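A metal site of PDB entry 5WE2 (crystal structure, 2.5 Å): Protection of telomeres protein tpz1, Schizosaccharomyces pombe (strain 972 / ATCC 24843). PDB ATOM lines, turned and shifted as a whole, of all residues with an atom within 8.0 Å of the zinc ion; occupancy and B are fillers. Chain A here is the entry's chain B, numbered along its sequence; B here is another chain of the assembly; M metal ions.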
ATOM      1  N   SER A   1      13.687  23.917  -9.623  1.00  0.00           N
ATOM      2  CA  SER A   1      12.423  23.379  -9.131  1.00  0.00           C
ATOM      3  C   SER A   1      11.647  22.807 -10.311  1.00  0.00           C
ATOM      4  O   SER A   1      12.255  22.295 -11.252  1.00  0.00           O
ATOM      5  CB  SER A   1      11.633  24.477  -8.411  1.00  0.00           C
ATOM      6  OG  SER A   1      12.352  24.976  -7.299  1.00  0.00           O
ATOM      7  N   GLU A   2      10.317  22.890 -10.260  1.00  0.00           N
ATOM      8  CA  GLU A   2       9.479  22.482 -11.384  1.00  0.00           C
ATOM      9  C   GLU A   2       9.601  23.479 -12.551  1.00  0.00           C
ATOM     10  O   GLU A   2      10.174  23.167 -13.600  1.00  0.00           O
ATOM     11  CB  GLU A   2       8.007  22.320 -10.932  1.00  0.00           C
ATOM     12  CG  GLU A   2       7.348  23.527 -10.206  1.00  0.00           C
ATOM     13  CD  GLU A   2       5.867  23.318  -9.885  1.00  0.00           C
ATOM     14  OE1 GLU A   2       5.538  22.415  -9.073  1.00  0.00           O
ATOM     15  OE2 GLU A   2       5.030  24.039 -10.480  1.00  0.00           O
ATOM     16  N   ALA A   3       9.066  24.682 -12.343  1.00  0.00           N
ATOM     17  CA  ALA A   3       9.185  25.781 -13.268  1.00  0.00           C
ATOM     18  C   ALA A   3       9.834  26.966 -12.546  1.00  0.00           C
ATOM     19  O   ALA A   3       9.155  27.897 -12.090  1.00  0.00           O
ATOM     20  CB  ALA A   3       7.834  26.169 -13.833  1.00  0.00           C
ATOM     21  N   CYS A   4      11.151  26.894 -12.417  1.00  0.00           N
ATOM     22  CA  CYS A   4      11.916  28.018 -11.937  1.00  0.00           C
ATOM     23  C   CYS A   4      12.150  28.959 -13.126  1.00  0.00           C
ATOM     24  O   CYS A   4      12.654  28.546 -14.164  1.00  0.00           O
ATOM     25  CB  CYS A   4      13.230  27.546 -11.317  1.00  0.00           C
ATOM     26  SG  CYS A   4      14.353  28.883 -10.931  1.00  0.00           S
ATOM     27  N   GLU A   5      11.767  30.221 -12.969  1.00  0.00           N
ATOM     28  CA  GLU A   5      11.920  31.202 -14.051  1.00  0.00           C
ATOM     29  C   GLU A   5      13.388  31.375 -14.454  1.00  0.00           C
ATOM     30  O   GLU A   5      13.691  31.715 -15.585  1.00  0.00           O
ATOM     31  CB  GLU A   5      11.317  32.568 -13.671  1.00  0.00           C
ATOM     32  CG  GLU A   5       9.795  32.550 -13.400  1.00  0.00           C
ATOM     33  CD  GLU A   5       8.987  31.970 -14.566  1.00  0.00           C
ATOM     34  OE1 GLU A   5       9.154  32.419 -15.731  1.00  0.00           O
ATOM     35  OE2 GLU A   5       8.198  31.040 -14.296  1.00  0.00           O
ATOM     36  N   MET A   6      14.296  31.134 -13.512  1.00  0.00           N
ATOM     37  CA  MET A   6      15.721  31.321 -13.788  1.00  0.00           C
ATOM     38  C   MET A   6      16.264  30.130 -14.577  1.00  0.00           C
ATOM     39  O   MET A   6      17.076  30.291 -15.489  1.00  0.00           O
ATOM     40  CB  MET A   6      16.485  31.516 -12.482  1.00  0.00           C
ATOM     41  CG  MET A   6      16.050  32.761 -11.733  1.00  0.00           C
ATOM     42  SD  MET A   6      16.420  34.224 -12.700  1.00  0.00           S
ATOM     43  CE  MET A   6      18.198  34.382 -12.394  1.00  0.00           C
ATOM     44  N   CYS A   7      15.793  28.941 -14.216  1.00  0.00           N
ATOM     45  CA  CYS A   7      16.063  27.730 -14.977  1.00  0.00           C
ATOM     46  C   CYS A   7      15.589  27.875 -16.452  1.00  0.00           C
ATOM     47  O   CYS A   7      16.406  27.818 -17.381  1.00  0.00           O
ATOM     48  CB  CYS A   7      15.437  26.497 -14.287  1.00  0.00           C
ATOM     49  SG  CYS A   7      16.444  25.867 -12.810  1.00  0.00           S
ATOM     50  N   ARG A   8      14.289  28.104 -16.656  1.00  0.00           N
ATOM     51  CA  ARG A   8      13.704  28.258 -17.994  1.00  0.00           C
ATOM     52  C   ARG A   8      14.520  29.172 -18.919  1.00  0.00           C
ATOM     53  O   ARG A   8      14.745  28.843 -20.095  1.00  0.00           O
ATOM     54  CB  ARG A   8      12.269  28.780 -17.871  1.00  0.00           C
ATOM     55  CG  ARG A   8      11.239  27.650 -17.732  1.00  0.00           C
ATOM     56  CD  ARG A   8       9.835  28.184 -17.690  1.00  0.00           C
ATOM     57  NE  ARG A   8       9.487  28.801 -18.971  1.00  0.00           N
ATOM     58  CZ  ARG A   8       8.962  28.146 -19.999  1.00  0.00           C
ATOM     59  NH1 ARG A   8       8.731  26.845 -19.907  1.00  0.00           N
ATOM     60  NH2 ARG A   8       8.673  28.789 -21.133  1.00  0.00           N
ATOM     61  N   LEU A   9      15.009  30.287 -18.384  1.00  0.00           N
ATOM     62  CA  LEU A   9      15.816  31.223 -19.151  1.00  0.00           C
ATOM     63  C   LEU A   9      17.279  30.828 -19.248  1.00  0.00           C
ATOM     64  O   LEU A   9      18.061  31.481 -19.954  1.00  0.00           O
ATOM     65  CB  LEU A   9      15.719  32.615 -18.548  1.00  0.00           C
ATOM     66  CG  LEU A   9      14.332  33.239 -18.495  1.00  0.00           C
ATOM     67  CD1 LEU A   9      14.384  34.445 -17.575  1.00  0.00           C
ATOM     68  CD2 LEU A   9      13.895  33.649 -19.916  1.00  0.00           C
ATOM     69  N   GLY A  10      17.685  29.802 -18.497  1.00  0.00           N
ATOM     70  CA  GLY A  10      19.089  29.438 -18.421  1.00  0.00           C
ATOM     71  C   GLY A  10      20.021  30.468 -17.760  1.00  0.00           C
ATOM     72  O   GLY A  10      21.194  30.575 -18.123  1.00  0.00           O
ATOM     73  N   LEU A  11      19.517  31.250 -16.821  1.00  0.00           N
ATOM     74  CA  LEU A  11      20.379  32.199 -16.121  1.00  0.00           C
ATOM     75  C   LEU A  11      21.019  31.519 -14.884  1.00  0.00           C
ATOM     76  O   LEU A  11      20.386  30.668 -14.252  1.00  0.00           O
ATOM     77  CB  LEU A  11      19.598  33.431 -15.705  1.00  0.00           C
ATOM     78  CG  LEU A  11      18.939  34.267 -16.806  1.00  0.00           C
ATOM     79  CD1 LEU A  11      17.988  35.238 -16.172  1.00  0.00           C
ATOM     80  CD2 LEU A  11      19.964  35.009 -17.658  1.00  0.00           C
ATOM     81  N   PRO A  12      22.267  31.891 -14.563  1.00  0.00           N
ATOM     82  CA  PRO A  12      22.886  31.327 -13.335  1.00  0.00           C
ATOM     83  C   PRO A  12      22.173  31.840 -12.092  1.00  0.00           C
ATOM     84  O   PRO A  12      21.887  33.020 -11.967  1.00  0.00           O
ATOM     85  CB  PRO A  12      24.349  31.837 -13.386  1.00  0.00           C
ATOM     86  CG  PRO A  12      24.258  33.168 -14.155  1.00  0.00           C
ATOM     87  CD  PRO A  12      23.088  32.967 -15.170  1.00  0.00           C
ATOM     88  N   HIS A  13      21.850  30.932 -11.205  1.00  0.00           N
ATOM     89  CA  HIS A  13      21.247  31.292  -9.925  1.00  0.00           C
ATOM     90  C   HIS A  13      21.591  30.198  -8.898  1.00  0.00           C
ATOM     91  O   HIS A  13      22.177  29.183  -9.270  1.00  0.00           O
ATOM     92  CB  HIS A  13      19.743  31.451 -10.055  1.00  0.00           C
ATOM     93  CG  HIS A  13      19.055  30.256 -10.669  1.00  0.00           C
ATOM     94  ND1 HIS A  13      19.276  29.846 -11.965  1.00  0.00           N
ATOM     95  CD2 HIS A  13      18.116  29.424 -10.155  1.00  0.00           C
ATOM     96  CE1 HIS A  13      18.509  28.793 -12.223  1.00  0.00           C
ATOM     97  NE2 HIS A  13      17.789  28.536 -11.151  1.00  0.00           N
ATOM     98  N   GLY A  14      21.247  30.400  -7.634  1.00  0.00           N
ATOM     99  CA  GLY A  14      21.390  29.312  -6.665  1.00  0.00           C
ATOM    100  C   GLY A  14      22.705  29.321  -5.902  1.00  0.00           C
ATOM    101  O   GLY A  14      23.559  30.190  -6.104  1.00  0.00           O
ATOM    102  N   LYS B  45      23.516  23.946 -14.731  1.00  0.00           N
ATOM    103  CA  LYS B  45      22.074  24.039 -14.565  1.00  0.00           C
ATOM    104  C   LYS B  45      21.586  23.011 -13.544  1.00  0.00           C
ATOM    105  O   LYS B  45      20.731  23.312 -12.699  1.00  0.00           O
ATOM    106  CB  LYS B  45      21.338  23.833 -15.899  1.00  0.00           C
ATOM    107  CG  LYS B  45      21.948  24.547 -17.109  1.00  0.00           C
ATOM    108  CD  LYS B  45      21.312  25.911 -17.350  1.00  0.00           C
ATOM    109  CE  LYS B  45      21.772  26.516 -18.681  1.00  0.00           C
ATOM    110  NZ  LYS B  45      21.281  25.744 -19.889  1.00  0.00           N
ATOM    111  N   MET B  47      23.004  21.850 -10.968  1.00  0.00           N
ATOM    112  CA  MET B  47      23.344  22.161  -9.586  1.00  0.00           C
ATOM    113  C   MET B  47      22.544  23.321  -9.029  1.00  0.00           C
ATOM    114  O   MET B  47      22.654  23.590  -7.827  1.00  0.00           O
ATOM    115  CB  MET B  47      24.860  22.472  -9.434  1.00  0.00           C
ATOM    116  CG  MET B  47      25.755  21.278  -9.784  1.00  0.00           C
ATOM    117  SD  MET B  47      25.275  19.754  -8.901  1.00  0.00           S
ATOM    118  CE  MET B  47      26.156  20.026  -7.363  1.00  0.00           C
ATOM    119  N   CYS B  48      21.722  23.967  -9.864  1.00  0.00           N
ATOM    120  CA  CYS B  48      21.025  25.185  -9.379  1.00  0.00           C
ATOM    121  C   CYS B  48      20.133  25.037  -8.129  1.00  0.00           C
ATOM    122  O   CYS B  48      19.842  26.010  -7.434  1.00  0.00           O
ATOM    123  CB  CYS B  48      20.162  25.780 -10.502  1.00  0.00           C
ATOM    124  SG  CYS B  48      21.167  26.615 -11.721  1.00  0.00           S
ATOM    125  N   HIS B  49      19.652  23.833  -7.880  1.00  0.00           N
ATOM    126  CA  HIS B  49      18.770  23.598  -6.745  1.00  0.00           C
ATOM    127  C   HIS B  49      19.281  22.450  -5.858  1.00  0.00           C
ATOM    128  O   HIS B  49      18.554  21.912  -5.029  1.00  0.00           O
ATOM    129  CB  HIS B  49      17.343  23.346  -7.246  1.00  0.00           C
ATOM    130  CG  HIS B  49      16.752  24.531  -7.937  1.00  0.00           C
ATOM    131  ND1 HIS B  49      16.015  25.491  -7.286  1.00  0.00           N
ATOM    132  CD2 HIS B  49      16.852  24.957  -9.222  1.00  0.00           C
ATOM    133  CE1 HIS B  49      15.672  26.441  -8.131  1.00  0.00           C
ATOM    134  NE2 HIS B  49      16.169  26.143  -9.321  1.00  0.00           N
HETATM  135 ZN    ZN M   1      16.141  27.389 -11.119  1.00  0.00          ZN
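SG of Cys 48 of chain B sits close to O of His 13, at 3.7 Å. A ring nitrogen (ND1) of His 13 lies within hydrogen-bond range of the backbone carbonyl oxygen (O) of Leu 11 (2.7 Å). NE2 of His 49 of chain B lies close to N of Ser 1, at 3.3 Å. N of Met 6 sits close to SG of Cys 4 (3.4 Å).
The zinc ion is bound by a ring nitrogen (NE2) of His 13. The zinc ion is bound by NE2 of His 49 of chain B (2.2 Å). SG of Cys 7 binds the zinc ion, 2.3 Å away. The side-chain sulfur (SG) of Cys 4 binds the zinc ion (2.3 Å).
The nearest printed residue that does not touch the zinc ion is Met 6 (4.4 Å).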
